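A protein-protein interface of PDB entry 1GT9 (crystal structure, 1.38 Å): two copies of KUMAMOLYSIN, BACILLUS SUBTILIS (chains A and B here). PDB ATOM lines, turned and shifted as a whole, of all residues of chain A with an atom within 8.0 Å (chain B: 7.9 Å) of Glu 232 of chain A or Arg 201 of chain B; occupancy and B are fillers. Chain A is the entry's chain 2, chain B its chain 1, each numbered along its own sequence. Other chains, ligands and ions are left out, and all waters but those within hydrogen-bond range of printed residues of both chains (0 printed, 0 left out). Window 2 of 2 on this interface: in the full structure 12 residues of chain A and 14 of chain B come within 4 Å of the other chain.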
ATOM      1  N   PHE A 225     -20.512  -2.207  -7.805  1.00  0.00           N
ATOM      2  CA  PHE A 225     -19.447  -3.196  -7.775  1.00  0.00           C
ATOM      3  C   PHE A 225     -18.074  -2.608  -7.799  1.00  0.00           C
ATOM      4  O   PHE A 225     -17.766  -1.779  -8.655  1.00  0.00           O
ATOM      5  CB  PHE A 225     -19.603  -4.140  -8.960  1.00  0.00           C
ATOM      6  CG  PHE A 225     -20.926  -4.878  -8.973  1.00  0.00           C
ATOM      7  CD1 PHE A 225     -21.960  -4.467  -9.807  1.00  0.00           C
ATOM      8  CD2 PHE A 225     -21.142  -5.957  -8.101  1.00  0.00           C
ATOM      9  CE1 PHE A 225     -23.183  -5.130  -9.767  1.00  0.00           C
ATOM     10  CE2 PHE A 225     -22.356  -6.611  -8.056  1.00  0.00           C
ATOM     11  CZ  PHE A 225     -23.378  -6.194  -8.895  1.00  0.00           C
ATOM     12  N   PRO A 226     -17.232  -2.988  -6.825  1.00  0.00           N
ATOM     13  CA  PRO A 226     -15.867  -2.453  -6.808  1.00  0.00           C
ATOM     14  C   PRO A 226     -15.113  -2.865  -8.077  1.00  0.00           C
ATOM     15  O   PRO A 226     -15.479  -3.824  -8.749  1.00  0.00           O
ATOM     16  CB  PRO A 226     -15.233  -3.128  -5.597  1.00  0.00           C
ATOM     17  CG  PRO A 226     -16.386  -3.454  -4.710  1.00  0.00           C
ATOM     18  CD  PRO A 226     -17.502  -3.857  -5.672  1.00  0.00           C
ATOM     19  N   LEU A 227     -14.036  -2.150  -8.368  1.00  0.00           N
ATOM     20  CA  LEU A 227     -13.165  -2.458  -9.505  1.00  0.00           C
ATOM     21  C   LEU A 227     -12.568  -3.852  -9.279  1.00  0.00           C
ATOM     22  O   LEU A 227     -11.864  -4.062  -8.292  1.00  0.00           O
ATOM     23  CB  LEU A 227     -12.040  -1.420  -9.526  1.00  0.00           C
ATOM     24  CG  LEU A 227     -11.037  -1.567 -10.679  1.00  0.00           C
ATOM     25  CD1 LEU A 227     -11.736  -1.382 -12.052  1.00  0.00           C
ATOM     26  CD2 LEU A 227      -9.950  -0.520 -10.538  1.00  0.00           C
ATOM     27  N   PRO A 228     -12.817  -4.813 -10.188  1.00  0.00           N
ATOM     28  CA  PRO A 228     -12.244  -6.160  -9.967  1.00  0.00           C
ATOM     29  C   PRO A 228     -10.725  -6.180 -10.077  1.00  0.00           C
ATOM     30  O   PRO A 228     -10.115  -5.423 -10.850  1.00  0.00           O
ATOM     31  CB  PRO A 228     -12.894  -7.026 -11.058  1.00  0.00           C
ATOM     32  CG  PRO A 228     -14.200  -6.300 -11.353  1.00  0.00           C
ATOM     33  CD  PRO A 228     -13.812  -4.830 -11.290  1.00  0.00           C
ATOM     34  N   SER A 229     -10.140  -7.111  -9.322  1.00  0.00           N
ATOM     35  CA  SER A 229      -8.697  -7.267  -9.337  1.00  0.00           C
ATOM     36  C   SER A 229      -8.188  -7.432 -10.756  1.00  0.00           C
ATOM     37  O   SER A 229      -7.184  -6.805 -11.125  1.00  0.00           O
ATOM     38  CB  SER A 229      -8.293  -8.463  -8.463  1.00  0.00           C
ATOM     39  OG  SER A 229      -8.954  -9.636  -8.880  1.00  0.00           O
ATOM     40  N   TRP A 230      -8.882  -8.221 -11.577  1.00  0.00           N
ATOM     41  CA  TRP A 230      -8.442  -8.473 -12.946  1.00  0.00           C
ATOM     42  C   TRP A 230      -8.642  -7.322 -13.879  1.00  0.00           C
ATOM     43  O   TRP A 230      -8.204  -7.376 -15.024  1.00  0.00           O
ATOM     44  CB  TRP A 230      -9.125  -9.731 -13.520  1.00  0.00           C
ATOM     45  CG  TRP A 230     -10.607  -9.807 -13.286  1.00  0.00           C
ATOM     46  CD1 TRP A 230     -11.215 -10.517 -12.306  1.00  0.00           C
ATOM     47  CD2 TRP A 230     -11.652  -9.121 -14.004  1.00  0.00           C
ATOM     48  NE1 TRP A 230     -12.573 -10.320 -12.347  1.00  0.00           N
ATOM     49  CE2 TRP A 230     -12.869  -9.466 -13.380  1.00  0.00           C
ATOM     50  CE3 TRP A 230     -11.676  -8.242 -15.092  1.00  0.00           C
ATOM     51  CZ2 TRP A 230     -14.115  -8.955 -13.815  1.00  0.00           C
ATOM     52  CZ3 TRP A 230     -12.906  -7.724 -15.526  1.00  0.00           C
ATOM     53  CH2 TRP A 230     -14.114  -8.090 -14.878  1.00  0.00           C
ATOM     54  N   GLN A 231      -9.298  -6.272 -13.407  1.00  0.00           N
ATOM     55  CA  GLN A 231      -9.563  -5.110 -14.241  1.00  0.00           C
ATOM     56  C   GLN A 231      -8.751  -3.896 -13.771  1.00  0.00           C
ATOM     57  O   GLN A 231      -8.871  -2.812 -14.325  1.00  0.00           O
ATOM     58  CB  GLN A 231     -11.071  -4.775 -14.200  1.00  0.00           C
ATOM     59  CG  GLN A 231     -11.535  -3.997 -15.433  1.00  0.00           C
ATOM     60  CD  GLN A 231     -13.006  -3.596 -15.384  1.00  0.00           C
ATOM     61  OE1 GLN A 231     -13.549  -3.238 -14.318  1.00  0.00           O
ATOM     62  NE2 GLN A 231     -13.651  -3.614 -16.552  1.00  0.00           N
ATOM     63  N   GLU A 232      -7.866  -4.090 -12.788  1.00  0.00           N
ATOM     64  CA  GLU A 232      -7.099  -2.950 -12.270  1.00  0.00           C
ATOM     65  C   GLU A 232      -6.015  -2.401 -13.181  1.00  0.00           C
ATOM     66  O   GLU A 232      -5.490  -1.331 -12.919  1.00  0.00           O
ATOM     67  CB  GLU A 232      -6.481  -3.296 -10.919  1.00  0.00           C
ATOM     68  CG  GLU A 232      -7.548  -3.470  -9.846  1.00  0.00           C
ATOM     69  CD  GLU A 232      -6.953  -3.674  -8.486  1.00  0.00           C
ATOM     70  OE1 GLU A 232      -7.469  -4.538  -7.729  1.00  0.00           O
ATOM     71  OE2 GLU A 232      -5.967  -2.962  -8.169  1.00  0.00           O
ATOM     72  N   ARG A 233      -5.678  -3.135 -14.228  1.00  0.00           N
ATOM     73  CA  ARG A 233      -4.658  -2.656 -15.163  1.00  0.00           C
ATOM     74  C   ARG A 233      -5.271  -2.157 -16.480  1.00  0.00           C
ATOM     75  O   ARG A 233      -4.570  -1.740 -17.390  1.00  0.00           O
ATOM     76  CB  ARG A 233      -3.637  -3.761 -15.429  1.00  0.00           C
ATOM     77  CG  ARG A 233      -2.658  -3.943 -14.240  1.00  0.00           C
ATOM     78  CD  ARG A 233      -1.945  -5.285 -14.338  1.00  0.00           C
ATOM     79  NE  ARG A 233      -2.906  -6.376 -14.203  1.00  0.00           N
ATOM     80  CZ  ARG A 233      -3.533  -6.664 -13.068  1.00  0.00           C
ATOM     81  NH1 ARG A 233      -4.418  -7.658 -13.030  1.00  0.00           N
ATOM     82  NH2 ARG A 233      -3.244  -5.976 -11.963  1.00  0.00           N
ATOM     83  N   ALA A 234      -6.598  -2.138 -16.550  1.00  0.00           N
ATOM     84  CA  ALA A 234      -7.303  -1.663 -17.742  1.00  0.00           C
ATOM     85  C   ALA A 234      -7.381  -0.154 -17.808  1.00  0.00           C
ATOM     86  O   ALA A 234      -7.722   0.406 -18.845  1.00  0.00           O
ATOM     87  CB  ALA A 234      -8.721  -2.199 -17.752  1.00  0.00           C
ATOM     88  N   ASN A 235      -7.089   0.512 -16.695  1.00  0.00           N
ATOM     89  CA  ASN A 235      -7.186   1.962 -16.611  1.00  0.00           C
ATOM     90  C   ASN A 235      -8.628   2.502 -16.709  1.00  0.00           C
ATOM     91  O   ASN A 235      -8.940   3.487 -17.415  1.00  0.00           O
ATOM     92  CB  ASN A 235      -6.250   2.631 -17.620  1.00  0.00           C
ATOM     93  CG  ASN A 235      -4.791   2.404 -17.260  1.00  0.00           C
ATOM     94  OD1 ASN A 235      -3.963   2.073 -18.111  1.00  0.00           O
ATOM     95  ND2 ASN A 235      -4.482   2.560 -15.982  1.00  0.00           N
ATOM     96  N   VAL A 236      -9.512   1.847 -15.953  1.00  0.00           N
ATOM     97  CA  VAL A 236     -10.899   2.295 -15.811  1.00  0.00           C
ATOM     98  C   VAL A 236     -10.773   3.663 -15.113  1.00  0.00           C
ATOM     99  O   VAL A 236     -10.103   3.793 -14.090  1.00  0.00           O
ATOM    100  CB  VAL A 236     -11.699   1.333 -14.923  1.00  0.00           C
ATOM    101  CG1 VAL A 236     -13.139   1.839 -14.738  1.00  0.00           C
ATOM    102  CG2 VAL A 236     -11.709  -0.066 -15.575  1.00  0.00           C
ATOM    103  N   SER A 246     -14.287   4.628  -7.550  1.00  0.00           N
ATOM    104  CA  SER A 246     -13.693   3.599  -8.382  1.00  0.00           C
ATOM    105  C   SER A 246     -14.759   2.517  -8.435  1.00  0.00           C
ATOM    106  O   SER A 246     -15.477   2.300  -7.459  1.00  0.00           O
ATOM    107  CB  SER A 246     -12.425   3.063  -7.708  1.00  0.00           C
ATOM    108  OG  SER A 246     -11.672   2.219  -8.560  1.00  0.00           O
ATOM    109  N   GLY A 247     -14.900   1.857  -9.569  1.00  0.00           N
ATOM    110  CA  GLY A 247     -15.875   0.788  -9.658  1.00  0.00           C
ATOM    111  C   GLY A 247     -15.617  -0.025 -10.911  1.00  0.00           C
ATOM    112  O   GLY A 247     -14.774   0.339 -11.761  1.00  0.00           O
ATOM    113  N   TYR A 307      -8.706  -9.968 -19.813  1.00  0.00           N
ATOM    114  CA  TYR A 307      -7.943  -8.791 -19.450  1.00  0.00           C
ATOM    115  C   TYR A 307      -6.437  -8.965 -19.342  1.00  0.00           C
ATOM    116  O   TYR A 307      -5.719  -8.010 -19.115  1.00  0.00           O
ATOM    117  CB  TYR A 307      -8.526  -8.150 -18.177  1.00  0.00           C
ATOM    118  CG  TYR A 307      -9.781  -7.357 -18.444  1.00  0.00           C
ATOM    119  CD1 TYR A 307     -11.013  -7.996 -18.567  1.00  0.00           C
ATOM    120  CD2 TYR A 307      -9.744  -5.965 -18.580  1.00  0.00           C
ATOM    121  CE1 TYR A 307     -12.178  -7.281 -18.809  1.00  0.00           C
ATOM    122  CE2 TYR A 307     -10.920  -5.233 -18.832  1.00  0.00           C
ATOM    123  CZ  TYR A 307     -12.124  -5.894 -18.941  1.00  0.00           C
ATOM    124  OH  TYR A 307     -13.284  -5.172 -19.134  1.00  0.00           O
ATOM    125  N   TYR B   6     -25.419  -8.117   0.203  1.00  0.00           N
ATOM    126  CA  TYR B   6     -24.616  -9.310  -0.007  1.00  0.00           C
ATOM    127  C   TYR B   6     -25.382 -10.535   0.427  1.00  0.00           C
ATOM    128  O   TYR B   6     -26.246 -10.452   1.292  1.00  0.00           O
ATOM    129  CB  TYR B   6     -23.370  -9.312   0.903  1.00  0.00           C
ATOM    130  CG  TYR B   6     -22.458  -8.137   0.766  1.00  0.00           C
ATOM    131  CD1 TYR B   6     -22.369  -7.171   1.766  1.00  0.00           C
ATOM    132  CD2 TYR B   6     -21.662  -8.001  -0.360  1.00  0.00           C
ATOM    133  CE1 TYR B   6     -21.490  -6.088   1.650  1.00  0.00           C
ATOM    134  CE2 TYR B   6     -20.800  -6.920  -0.495  1.00  0.00           C
ATOM    135  CZ  TYR B   6     -20.716  -5.971   0.514  1.00  0.00           C
ATOM    136  OH  TYR B   6     -19.851  -4.907   0.393  1.00  0.00           O
ATOM    137  N   ASP B  10     -21.187 -14.199   0.563  1.00  0.00           N
ATOM    138  CA  ASP B  10     -20.258 -13.161   0.131  1.00  0.00           C
ATOM    139  C   ASP B  10     -19.527 -12.563   1.327  1.00  0.00           C
ATOM    140  O   ASP B  10     -18.334 -12.292   1.249  1.00  0.00           O
ATOM    141  CB  ASP B  10     -20.995 -12.064  -0.650  1.00  0.00           C
ATOM    142  CG  ASP B  10     -21.735 -12.619  -1.841  1.00  0.00           C
ATOM    143  OD1 ASP B  10     -22.969 -12.456  -1.926  1.00  0.00           O
ATOM    144  OD2 ASP B  10     -21.095 -13.258  -2.697  1.00  0.00           O
ATOM    145  N   GLN B  13     -16.939 -14.991   2.596  1.00  0.00           N
ATOM    146  CA  GLN B  13     -15.809 -15.007   1.672  1.00  0.00           C
ATOM    147  C   GLN B  13     -14.888 -13.813   1.962  1.00  0.00           C
ATOM    148  O   GLN B  13     -13.664 -13.961   2.040  1.00  0.00           O
ATOM    149  CB  GLN B  13     -16.322 -14.967   0.226  1.00  0.00           C
ATOM    150  CG  GLN B  13     -15.220 -14.794  -0.825  1.00  0.00           C
ATOM    151  CD  GLN B  13     -14.407 -16.256  -0.786  1.00  0.00           C
ATOM    152  OE1 GLN B  13     -14.931 -17.376  -0.827  1.00  0.00           O
ATOM    153  NE2 GLN B  13     -13.082 -16.077  -0.696  1.00  0.00           N
ATOM    154  N   ALA B  14     -15.487 -12.635   2.139  1.00  0.00           N
ATOM    155  CA  ALA B  14     -14.721 -11.430   2.427  1.00  0.00           C
ATOM    156  C   ALA B  14     -13.912 -11.586   3.719  1.00  0.00           C
ATOM    157  O   ALA B  14     -12.797 -11.102   3.793  1.00  0.00           O
ATOM    158  CB  ALA B  14     -15.646 -10.224   2.556  1.00  0.00           C
ATOM    159  N   TYR B  15     -14.480 -12.263   4.720  1.00  0.00           N
ATOM    160  CA  TYR B  15     -13.805 -12.487   5.990  1.00  0.00           C
ATOM    161  C   TYR B  15     -12.996 -13.770   5.995  1.00  0.00           C
ATOM    162  O   TYR B  15     -12.570 -14.244   7.041  1.00  0.00           O
ATOM    163  CB  TYR B  15     -14.830 -12.510   7.129  1.00  0.00           C
ATOM    164  CG  TYR B  15     -15.498 -11.179   7.365  1.00  0.00           C
ATOM    165  CD1 TYR B  15     -16.787 -11.120   7.878  1.00  0.00           C
ATOM    166  CD2 TYR B  15     -14.824  -9.981   7.092  1.00  0.00           C
ATOM    167  CE1 TYR B  15     -17.399  -9.914   8.124  1.00  0.00           C
ATOM    168  CE2 TYR B  15     -15.423  -8.753   7.335  1.00  0.00           C
ATOM    169  CZ  TYR B  15     -16.716  -8.737   7.855  1.00  0.00           C
ATOM    170  OH  TYR B  15     -17.339  -7.549   8.105  1.00  0.00           O
ATOM    171  N   GLN B  16     -12.796 -14.346   4.815  1.00  0.00           N
ATOM    172  CA  GLN B  16     -11.981 -15.549   4.688  1.00  0.00           C
ATOM    173  C   GLN B  16     -12.343 -16.676   5.666  1.00  0.00           C
ATOM    174  O   GLN B  16     -11.477 -17.237   6.371  1.00  0.00           O
ATOM    175  CB  GLN B  16     -10.497 -15.175   4.816  1.00  0.00           C
ATOM    176  CG  GLN B  16     -10.041 -14.174   3.747  1.00  0.00           C
ATOM    177  CD  GLN B  16      -8.627 -13.683   3.993  1.00  0.00           C
ATOM    178  OE1 GLN B  16      -8.414 -12.543   4.397  1.00  0.00           O
ATOM    179  NE2 GLN B  16      -7.662 -14.550   3.774  1.00  0.00           N
ATOM    180  N   LEU B 195     -19.249  -2.719   5.331  1.00  0.00           N
ATOM    181  CA  LEU B 195     -18.268  -3.485   4.568  1.00  0.00           C
ATOM    182  C   LEU B 195     -18.427  -3.329   3.065  1.00  0.00           C
ATOM    183  O   LEU B 195     -19.525  -3.541   2.543  1.00  0.00           O
ATOM    184  CB  LEU B 195     -18.416  -4.976   4.924  1.00  0.00           C
ATOM    185  CG  LEU B 195     -17.481  -5.918   4.162  1.00  0.00           C
ATOM    186  CD1 LEU B 195     -16.063  -5.730   4.676  1.00  0.00           C
ATOM    187  CD2 LEU B 195     -17.940  -7.366   4.325  1.00  0.00           C
ATOM    188  N   VAL B 196     -17.341  -2.966   2.387  1.00  0.00           N
ATOM    189  CA  VAL B 196     -17.329  -2.877   0.935  1.00  0.00           C
ATOM    190  C   VAL B 196     -16.295  -3.940   0.588  1.00  0.00           C
ATOM    191  O   VAL B 196     -15.080  -3.788   0.872  1.00  0.00           O
ATOM    192  CB  VAL B 196     -16.866  -1.520   0.401  1.00  0.00           C
ATOM    193  CG1 VAL B 196     -16.824  -1.571  -1.137  1.00  0.00           C
ATOM    194  CG2 VAL B 196     -17.798  -0.437   0.851  1.00  0.00           C
ATOM    195  N   ALA B 197     -16.771  -5.042   0.023  1.00  0.00           N
ATOM    196  CA  ALA B 197     -15.894  -6.154  -0.295  1.00  0.00           C
ATOM    197  C   ALA B 197     -16.358  -6.891  -1.509  1.00  0.00           C
ATOM    198  O   ALA B 197     -17.518  -6.801  -1.891  1.00  0.00           O
ATOM    199  CB  ALA B 197     -15.830  -7.131   0.896  1.00  0.00           C
ATOM    200  N   SER B 198     -15.419  -7.605  -2.124  1.00  0.00           N
ATOM    201  CA  SER B 198     -15.702  -8.442  -3.283  1.00  0.00           C
ATOM    202  C   SER B 198     -15.090  -9.795  -2.942  1.00  0.00           C
ATOM    203  O   SER B 198     -14.523  -9.954  -1.862  1.00  0.00           O
ATOM    204  CB  SER B 198     -15.112  -7.827  -4.557  1.00  0.00           C
ATOM    205  OG  SER B 198     -13.771  -7.424  -4.353  1.00  0.00           O
ATOM    206  N   ALA B 199     -15.197 -10.778  -3.826  1.00  0.00           N
ATOM    207  CA  ALA B 199     -14.688 -12.108  -3.479  1.00  0.00           C
ATOM    208  C   ALA B 199     -13.228 -12.203  -3.045  1.00  0.00           C
ATOM    209  O   ALA B 199     -12.896 -12.992  -2.158  1.00  0.00           O
ATOM    210  CB  ALA B 199     -14.921 -13.083  -4.632  1.00  0.00           C
ATOM    211  N   GLY B 200     -12.363 -11.400  -3.654  1.00  0.00           N
ATOM    212  CA  GLY B 200     -10.947 -11.490  -3.339  1.00  0.00           C
ATOM    213  C   GLY B 200     -10.351 -10.512  -2.356  1.00  0.00           C
ATOM    214  O   GLY B 200      -9.224 -10.734  -1.912  1.00  0.00           O
ATOM    215  N   ARG B 201     -11.062  -9.435  -2.011  1.00  0.00           N
ATOM    216  CA  ARG B 201     -10.515  -8.449  -1.077  1.00  0.00           C
ATOM    217  C   ARG B 201     -11.580  -7.580  -0.428  1.00  0.00           C
ATOM    218  O   ARG B 201     -12.731  -7.543  -0.880  1.00  0.00           O
ATOM    219  CB  ARG B 201      -9.521  -7.538  -1.809  1.00  0.00           C
ATOM    220  CG  ARG B 201     -10.167  -6.509  -2.754  1.00  0.00           C
ATOM    221  CD  ARG B 201      -9.109  -5.851  -3.650  1.00  0.00           C
ATOM    222  NE  ARG B 201      -9.558  -4.587  -4.255  1.00  0.00           N
ATOM    223  CZ  ARG B 201     -10.210  -4.495  -5.410  1.00  0.00           C
ATOM    224  NH1 ARG B 201     -10.511  -5.594  -6.114  1.00  0.00           N
ATOM    225  NH2 ARG B 201     -10.519  -3.286  -5.880  1.00  0.00           N
ATOM    226  N   ILE B 202     -11.185  -6.899   0.642  1.00  0.00           N
ATOM    227  CA  ILE B 202     -12.049  -5.960   1.334  1.00  0.00           C
ATOM    228  C   ILE B 202     -11.543  -4.624   0.820  1.00  0.00           C
ATOM    229  O   ILE B 202     -10.388  -4.262   1.041  1.00  0.00           O
ATOM    230  CB  ILE B 202     -11.877  -6.003   2.887  1.00  0.00           C
ATOM    231  CG1 ILE B 202     -12.385  -7.353   3.410  1.00  0.00           C
ATOM    232  CG2 ILE B 202     -12.586  -4.796   3.548  1.00  0.00           C
ATOM    233  CD1 ILE B 202     -13.866  -7.442   3.572  1.00  0.00           C
ATOM    234  N   GLU B 203     -12.399  -3.906   0.109  1.00  0.00           N
ATOM    235  CA  GLU B 203     -12.005  -2.591  -0.371  1.00  0.00           C
ATOM    236  C   GLU B 203     -12.067  -1.547   0.744  1.00  0.00           C
ATOM    237  O   GLU B 203     -11.263  -0.630   0.782  1.00  0.00           O
ATOM    238  CB  GLU B 203     -12.886  -2.151  -1.538  1.00  0.00           C
ATOM    239  CG  GLU B 203     -12.557  -2.896  -2.850  1.00  0.00           C
ATOM    240  CD  GLU B 203     -13.268  -4.229  -3.018  1.00  0.00           C
ATOM    241  OE1 GLU B 203     -14.260  -4.508  -2.308  1.00  0.00           O
ATOM    242  OE2 GLU B 203     -12.857  -5.027  -3.897  1.00  0.00           O
ATOM    243  N   ARG B 204     -13.032  -1.671   1.660  1.00  0.00           N
ATOM    244  CA  ARG B 204     -13.162  -0.686   2.739  1.00  0.00           C
ATOM    245  C   ARG B 204     -14.021  -1.255   3.858  1.00  0.00           C
ATOM    246  O   ARG B 204     -14.996  -1.943   3.587  1.00  0.00           O
ATOM    247  CB  ARG B 204     -13.830   0.599   2.214  1.00  0.00           C
ATOM    248  CG  ARG B 204     -13.757   1.796   3.134  1.00  0.00           C
ATOM    249  CD  ARG B 204     -14.311   3.031   2.417  1.00  0.00           C
ATOM    250  NE  ARG B 204     -14.300   4.237   3.244  1.00  0.00           N
ATOM    251  CZ  ARG B 204     -13.214   4.782   3.784  1.00  0.00           C
ATOM    252  NH1 ARG B 204     -13.336   5.884   4.509  1.00  0.00           N
ATOM    253  NH2 ARG B 204     -12.018   4.234   3.618  1.00  0.00           N
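Of the 16 printed residues of chain B, 2 touch a printed residue of chain A. Of the 15 printed residues of chain A, 4 touch a printed residue of chain B. Hydrophobic or aromatic side chains of chain A within 4 Å of the printed part of chain B: Pro 226. Among the printed residues, 4 pairs touch across the chains.
Of the printed residues of chain B, Pro 226 of chain A touches Glu 203 (3.4 Å). Of the printed residues of chain B, Leu 227 of chain A touches Arg 201. Of the printed residues of chain B, Ser 229 of chain A touches Arg 201 (3.6 Å). Arg 233 of chain A touches none of the printed residues of chain B. Of the printed residues of chain A, Arg 201 of chain B touches Leu 227 (2.9 Å), Ser 229 (3.6 Å) and Glu 232 (3.6 Å). Of the printed residues of chain A, Glu 203 of chain B touches Pro 226. The nearest residue of chain B that does not touch Glu 232 of chain A is Glu 203 of chain B (6.6 Å). The nearest printed residue of chain A that does not touch Arg 201 of chain B is Pro 228 of chain A (4.01 Å). The nearest printed residue of chain B that does not touch Pro 226 of chain A is Val 196 of chain B (4.1 Å).
NH2 of Arg 201 of chain B is in hydrogen-bond range of O of Leu 227 of chain A, 2.9 Å away. The side-chain carboxylate (OE1) of Glu 232 of chain A is in salt-bridge range of the guanidinium group (NH1) of Arg 201 of chain B (3.6 Å).
No position is printed for both chains. Of the 4 pairs that touch across the chains among the printed residues, none has its exchanged pair printed and touching as well.
Among the printed residues, pairs that only touch across the chains: Pro 226 of chain A with Glu 203 of chain B (3.4 Å) and Ser 229 of chain A with Arg 201 of chain B (3.6 Å).
The side-chain hydroxyl (OG) of Ser 198 of chain B is in hydrogen-bond range of the side-chain carboxylate (OE2) of Glu 203 of chain B (2.6 Å). The side-chain carboxylate of Glu 203 of chain B lies within salt-bridge range of the guanidinium group of Arg 201 of chain B (3.3 Å). O of Ser 229 of chain A sits at hydrogen-bond distance from NH1 of Arg 233 of chain A, at 3.5 Å. O of Val 196 of chain B lies within hydrogen-bond range of N of Glu 203 of chain B (2.8 Å). OE1 of Glu 203 of chain B sits close to N of Ala 197 of chain B, at 3.5 Å.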
